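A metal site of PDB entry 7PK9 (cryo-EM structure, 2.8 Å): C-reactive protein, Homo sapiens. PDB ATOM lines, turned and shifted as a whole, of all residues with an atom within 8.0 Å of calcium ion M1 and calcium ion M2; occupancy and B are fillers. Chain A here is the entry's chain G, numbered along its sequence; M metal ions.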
ATOM      1  N   SER A  50      19.154 -20.572  25.950  1.00  0.00           N
ATOM      2  CA  SER A  50      19.638 -21.944  25.866  1.00  0.00           C
ATOM      3  C   SER A  50      20.974 -22.101  25.133  1.00  0.00           C
ATOM      4  O   SER A  50      21.084 -21.776  23.954  1.00  0.00           O
ATOM      5  CB  SER A  50      18.593 -22.806  25.175  1.00  0.00           C
ATOM      6  OG  SER A  50      18.942 -24.179  25.298  1.00  0.00           O
ATOM      7  N   SER A  53      20.495 -27.907  25.136  1.00  0.00           N
ATOM      8  CA  SER A  53      19.215 -28.445  25.557  1.00  0.00           C
ATOM      9  C   SER A  53      19.172 -29.944  25.240  1.00  0.00           C
ATOM     10  O   SER A  53      19.205 -30.347  24.075  1.00  0.00           O
ATOM     11  CB  SER A  53      18.075 -27.700  24.871  1.00  0.00           C
ATOM     12  OG  SER A  53      16.824 -28.069  25.405  1.00  0.00           O
ATOM     13  N   ALA A  55      16.844 -33.222  26.076  1.00  0.00           N
ATOM     14  CA  ALA A  55      15.514 -33.578  26.559  1.00  0.00           C
ATOM     15  C   ALA A  55      15.189 -35.029  26.241  1.00  0.00           C
ATOM     16  O   ALA A  55      15.641 -35.590  25.243  1.00  0.00           O
ATOM     17  CB  ALA A  55      14.439 -32.716  25.921  1.00  0.00           C
ATOM     18  N   GLN A  59      11.456 -35.960  30.398  1.00  0.00           N
ATOM     19  CA  GLN A  59      11.993 -34.739  31.011  1.00  0.00           C
ATOM     20  C   GLN A  59      12.550 -33.847  29.918  1.00  0.00           C
ATOM     21  O   GLN A  59      13.531 -34.215  29.261  1.00  0.00           O
ATOM     22  CB  GLN A  59      13.072 -35.122  32.010  1.00  0.00           C
ATOM     23  CG  GLN A  59      13.786 -33.973  32.662  1.00  0.00           C
ATOM     24  CD  GLN A  59      12.832 -32.987  33.283  1.00  0.00           C
ATOM     25  OE1 GLN A  59      12.575 -31.919  32.726  1.00  0.00           O
ATOM     26  NE2 GLN A  59      12.291 -33.345  34.439  1.00  0.00           N
ATOM     27  N   ASP A  60      11.920 -32.685  29.705  1.00  0.00           N
ATOM     28  CA  ASP A  60      12.347 -31.768  28.663  1.00  0.00           C
ATOM     29  C   ASP A  60      13.641 -31.052  29.010  1.00  0.00           C
ATOM     30  O   ASP A  60      14.335 -30.585  28.095  1.00  0.00           O
ATOM     31  CB  ASP A  60      11.264 -30.733  28.370  1.00  0.00           C
ATOM     32  CG  ASP A  60      10.974 -29.834  29.539  1.00  0.00           C
ATOM     33  OD1 ASP A  60      11.578 -30.042  30.610  1.00  0.00           O
ATOM     34  OD2 ASP A  60      10.143 -28.910  29.404  1.00  0.00           O
ATOM     35  N   ASN A  61      13.988 -30.949  30.286  1.00  0.00           N
ATOM     36  CA  ASN A  61      15.229 -30.318  30.703  1.00  0.00           C
ATOM     37  C   ASN A  61      16.160 -31.355  31.316  1.00  0.00           C
ATOM     38  O   ASN A  61      16.584 -31.218  32.465  1.00  0.00           O
ATOM     39  CB  ASN A  61      14.965 -29.212  31.729  1.00  0.00           C
ATOM     40  CG  ASN A  61      14.167 -28.077  31.161  1.00  0.00           C
ATOM     41  OD1 ASN A  61      14.336 -27.705  29.995  1.00  0.00           O
ATOM     42  ND2 ASN A  61      13.315 -27.486  31.979  1.00  0.00           N
ATOM     43  N   GLU A  62      16.460 -32.402  30.559  1.00  0.00           N
ATOM     44  CA  GLU A  62      17.252 -33.491  31.109  1.00  0.00           C
ATOM     45  C   GLU A  62      18.709 -33.097  31.264  1.00  0.00           C
ATOM     46  O   GLU A  62      19.357 -33.466  32.250  1.00  0.00           O
ATOM     47  CB  GLU A  62      17.077 -34.724  30.239  1.00  0.00           C
ATOM     48  CG  GLU A  62      17.814 -35.932  30.733  1.00  0.00           C
ATOM     49  CD  GLU A  62      17.255 -36.421  32.045  1.00  0.00           C
ATOM     50  OE1 GLU A  62      16.070 -36.158  32.310  1.00  0.00           O
ATOM     51  OE2 GLU A  62      17.970 -37.109  32.791  1.00  0.00           O
ATOM     52  N   LEU A  64      20.278 -29.089  30.714  1.00  0.00           N
ATOM     53  CA  LEU A  64      20.130 -27.712  30.240  1.00  0.00           C
ATOM     54  C   LEU A  64      21.339 -26.929  30.713  1.00  0.00           C
ATOM     55  O   LEU A  64      21.506 -26.723  31.918  1.00  0.00           O
ATOM     56  CB  LEU A  64      18.826 -27.086  30.729  1.00  0.00           C
ATOM     57  CG  LEU A  64      18.375 -25.811  30.035  1.00  0.00           C
ATOM     58  CD1 LEU A  64      18.151 -25.960  28.537  1.00  0.00           C
ATOM     59  CD2 LEU A  64      17.136 -25.286  30.703  1.00  0.00           C
ATOM     60  N   PHE A  66      22.144 -23.226  30.545  1.00  0.00           N
ATOM     61  CA  PHE A  66      21.324 -22.054  30.295  1.00  0.00           C
ATOM     62  C   PHE A  66      21.961 -20.827  30.946  1.00  0.00           C
ATOM     63  O   PHE A  66      22.160 -20.805  32.158  1.00  0.00           O
ATOM     64  CB  PHE A  66      19.915 -22.260  30.835  1.00  0.00           C
ATOM     65  CG  PHE A  66      18.894 -21.336  30.267  1.00  0.00           C
ATOM     66  CD1 PHE A  66      18.088 -21.730  29.219  1.00  0.00           C
ATOM     67  CD2 PHE A  66      18.701 -20.087  30.822  1.00  0.00           C
ATOM     68  CE1 PHE A  66      17.145 -20.876  28.716  1.00  0.00           C
ATOM     69  CE2 PHE A  66      17.758 -19.233  30.319  1.00  0.00           C
ATOM     70  CZ  PHE A  66      16.971 -19.625  29.260  1.00  0.00           C
ATOM     71  N   THR A  76      21.335 -27.658  34.781  1.00  0.00           N
ATOM     72  CA  THR A  76      20.241 -28.465  35.310  1.00  0.00           C
ATOM     73  C   THR A  76      20.340 -29.862  34.760  1.00  0.00           C
ATOM     74  O   THR A  76      20.582 -30.062  33.569  1.00  0.00           O
ATOM     75  CB  THR A  76      18.856 -27.926  34.918  1.00  0.00           C
ATOM     76  OG1 THR A  76      18.655 -28.118  33.515  1.00  0.00           O
ATOM     77  CG2 THR A  76      18.743 -26.480  35.198  1.00  0.00           C
ATOM     78  N   GLN A 137      17.857 -23.627  20.691  1.00  0.00           N
ATOM     79  CA  GLN A 137      16.549 -23.519  21.293  1.00  0.00           C
ATOM     80  C   GLN A 137      16.587 -24.205  22.648  1.00  0.00           C
ATOM     81  O   GLN A 137      17.353 -25.148  22.855  1.00  0.00           O
ATOM     82  CB  GLN A 137      15.450 -24.145  20.435  1.00  0.00           C
ATOM     83  CG  GLN A 137      15.352 -23.605  19.035  1.00  0.00           C
ATOM     84  CD  GLN A 137      15.000 -22.121  19.002  1.00  0.00           C
ATOM     85  OE1 GLN A 137      14.473 -21.586  19.973  1.00  0.00           O
ATOM     86  NE2 GLN A 137      15.265 -21.478  17.883  1.00  0.00           N
ATOM     87  N   GLU A 138      15.747 -23.744  23.557  1.00  0.00           N
ATOM     88  CA  GLU A 138      15.339 -24.538  24.713  1.00  0.00           C
ATOM     89  C   GLU A 138      14.080 -25.307  24.343  1.00  0.00           C
ATOM     90  O   GLU A 138      13.074 -24.714  23.952  1.00  0.00           O
ATOM     91  CB  GLU A 138      15.126 -23.637  25.917  1.00  0.00           C
ATOM     92  CG  GLU A 138      15.240 -24.346  27.246  1.00  0.00           C
ATOM     93  CD  GLU A 138      13.926 -24.927  27.670  1.00  0.00           C
ATOM     94  OE1 GLU A 138      12.905 -24.244  27.461  1.00  0.00           O
ATOM     95  OE2 GLU A 138      13.896 -26.062  28.195  1.00  0.00           O
ATOM     96  N   GLN A 139      14.137 -26.638  24.467  1.00  0.00           N
ATOM     97  CA  GLN A 139      13.010 -27.480  24.137  1.00  0.00           C
ATOM     98  C   GLN A 139      12.215 -27.816  25.398  1.00  0.00           C
ATOM     99  O   GLN A 139      12.784 -28.221  26.411  1.00  0.00           O
ATOM    100  CB  GLN A 139      13.427 -28.769  23.413  1.00  0.00           C
ATOM    101  CG  GLN A 139      14.095 -29.853  24.225  1.00  0.00           C
ATOM    102  CD  GLN A 139      15.025 -30.707  23.377  1.00  0.00           C
ATOM    103  OE1 GLN A 139      14.577 -31.437  22.513  1.00  0.00           O
ATOM    104  NE2 GLN A 139      16.314 -30.655  23.651  1.00  0.00           N
ATOM    105  N   ASP A 140      10.902 -27.607  25.317  1.00  0.00           N
ATOM    106  CA  ASP A 140       9.975 -27.839  26.419  1.00  0.00           C
ATOM    107  C   ASP A 140       9.051 -29.013  26.179  1.00  0.00           C
ATOM    108  O   ASP A 140       8.334 -29.411  27.106  1.00  0.00           O
ATOM    109  CB  ASP A 140       9.127 -26.593  26.681  1.00  0.00           C
ATOM    110  CG  ASP A 140       9.918 -25.467  27.262  1.00  0.00           C
ATOM    111  OD1 ASP A 140      11.112 -25.684  27.504  1.00  0.00           O
ATOM    112  OD2 ASP A 140       9.358 -24.378  27.493  1.00  0.00           O
ATOM    113  N   SER A 141       9.035 -29.556  24.981  1.00  0.00           N
ATOM    114  CA  SER A 141       8.568 -30.907  24.737  1.00  0.00           C
ATOM    115  C   SER A 141       9.781 -31.751  24.384  1.00  0.00           C
ATOM    116  O   SER A 141      10.933 -31.299  24.475  1.00  0.00           O
ATOM    117  CB  SER A 141       7.529 -30.905  23.627  1.00  0.00           C
ATOM    118  OG  SER A 141       8.094 -30.396  22.428  1.00  0.00           O
ATOM    119  N   GLY A 144      10.410 -29.946  20.782  1.00  0.00           N
ATOM    120  CA  GLY A 144       9.718 -28.762  20.325  1.00  0.00           C
ATOM    121  C   GLY A 144       9.306 -27.849  21.458  1.00  0.00           C
ATOM    122  O   GLY A 144       9.863 -27.914  22.560  1.00  0.00           O
ATOM    123  N   ASN A 145       8.304 -27.019  21.179  1.00  0.00           N
ATOM    124  CA  ASN A 145       7.815 -26.012  22.121  1.00  0.00           C
ATOM    125  C   ASN A 145       8.906 -25.004  22.477  1.00  0.00           C
ATOM    126  O   ASN A 145       9.020 -24.561  23.616  1.00  0.00           O
ATOM    127  CB  ASN A 145       7.262 -26.659  23.390  1.00  0.00           C
ATOM    128  CG  ASN A 145       6.121 -27.606  23.104  1.00  0.00           C
ATOM    129  OD1 ASN A 145       6.282 -28.607  22.405  1.00  0.00           O
ATOM    130  ND2 ASN A 145       4.963 -27.303  23.657  1.00  0.00           N
ATOM    131  N   PHE A 146       9.710 -24.646  21.487  1.00  0.00           N
ATOM    132  CA  PHE A 146      10.730 -23.621  21.644  1.00  0.00           C
ATOM    133  C   PHE A 146      10.097 -22.267  21.976  1.00  0.00           C
ATOM    134  O   PHE A 146       8.930 -22.018  21.725  1.00  0.00           O
ATOM    135  CB  PHE A 146      11.604 -23.532  20.394  1.00  0.00           C
ATOM    136  CG  PHE A 146      11.945 -24.862  19.790  1.00  0.00           C
ATOM    137  CD1 PHE A 146      12.589 -25.822  20.543  1.00  0.00           C
ATOM    138  CD2 PHE A 146      11.617 -25.156  18.495  1.00  0.00           C
ATOM    139  CE1 PHE A 146      12.920 -27.036  20.009  1.00  0.00           C
ATOM    140  CE2 PHE A 146      11.930 -26.364  17.948  1.00  0.00           C
ATOM    141  CZ  PHE A 146      12.580 -27.313  18.706  1.00  0.00           C
ATOM    142  N   GLU A 147      10.909 -21.403  22.581  1.00  0.00           N
ATOM    143  CA  GLU A 147      10.513 -20.031  22.924  1.00  0.00           C
ATOM    144  C   GLU A 147      11.536 -19.069  22.348  1.00  0.00           C
ATOM    145  O   GLU A 147      12.719 -19.147  22.664  1.00  0.00           O
ATOM    146  CB  GLU A 147      10.404 -19.862  24.433  1.00  0.00           C
ATOM    147  CG  GLU A 147       9.363 -20.761  25.070  1.00  0.00           C
ATOM    148  CD  GLU A 147       9.611 -20.961  26.550  1.00  0.00           C
ATOM    149  OE1 GLU A 147       9.952 -22.096  26.924  1.00  0.00           O
ATOM    150  OE2 GLU A 147       9.461 -19.994  27.315  1.00  0.00           O
ATOM    151  N   SER A 149      12.197 -15.959  22.967  1.00  0.00           N
ATOM    152  CA  SER A 149      12.954 -15.334  24.043  1.00  0.00           C
ATOM    153  C   SER A 149      14.077 -16.210  24.608  1.00  0.00           C
ATOM    154  O   SER A 149      14.905 -15.691  25.363  1.00  0.00           O
ATOM    155  CB  SER A 149      12.015 -14.951  25.175  1.00  0.00           C
ATOM    156  OG  SER A 149      11.421 -16.105  25.739  1.00  0.00           O
ATOM    157  N   GLN A 150      14.107 -17.500  24.292  1.00  0.00           N
ATOM    158  CA  GLN A 150      15.135 -18.411  24.777  1.00  0.00           C
ATOM    159  C   GLN A 150      16.023 -18.959  23.680  1.00  0.00           C
ATOM    160  O   GLN A 150      16.939 -19.731  23.977  1.00  0.00           O
ATOM    161  CB  GLN A 150      14.493 -19.543  25.565  1.00  0.00           C
ATOM    162  CG  GLN A 150      13.641 -19.064  26.699  1.00  0.00           C
ATOM    163  CD  GLN A 150      13.208 -20.186  27.598  1.00  0.00           C
ATOM    164  OE1 GLN A 150      13.041 -21.318  27.165  1.00  0.00           O
ATOM    165  NE2 GLN A 150      13.061 -19.885  28.876  1.00  0.00           N
HETATM  166 CA    CA M   1      12.169 -26.441  29.554  1.00  0.00          CA
HETATM  167 CA    CA M   2      11.604 -22.617  28.189  1.00  0.00          CA
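OD2 of Asp 140 sits close to OE1 of Glu 147. O of Gln 150 lies within hydrogen-bond range of N of Ser 50 (3.1 Å). OD1 of Asp 60 sits close to ND2 of Asn 61 (3.4 Å). The side-chain amide oxygen of Gln 59 sits at hydrogen-bond distance from the backbone NH of Asn 61. The side-chain carboxylate of Asp 60 sits close to the side-chain amide oxygen of Gln 59, 3.0 Å away. NE2 of Gln 139 lies within hydrogen-bond range of O of Ser 53, at 2.9 Å.
OD2 of Asp 60 touches calcium ion M1, 3.2 Å away. O of Gln 139 touches calcium ion M1, 3.7 Å away. Within 4 Å of calcium ion M1: Asp 60, Asn 61, Glu 138, Gln 139 and Asp 140. The nearest printed residue that does not touch calcium ion M1 is Leu 64 (5.2 Å).
Within 4 Å of calcium ion M2: Glu 138, Asp 140, Glu 147 and Gln 150.
Calcium ion M1 is bound by the side-chain carboxylate (OE2) of Glu 138 (2.2 Å). OD1 of Asp 140 is bound to calcium ion M1, at 2.4 Å. OD1 of Asn 61 binds calcium ion M1 (2.5 Å). ND2 of Asn 61 binds calcium ion M1 (2.9 Å). Calcium ion M1 has four donor atoms within binding distance. Slightly farther from calcium ion M1 lies OE1 of Glu 138 (3.1 Å).
Calcium ion M2 is bound by OE1 of Glu 147, at 2.1 Å. OE1 of Gln 150 binds calcium ion M2 (2.2 Å). OE1 of Glu 138 binds calcium ion M2 (2.2 Å). Slightly farther from calcium ion M2 lies the side-chain carboxylate (OD2) of Asp 140 (2.9 Å).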
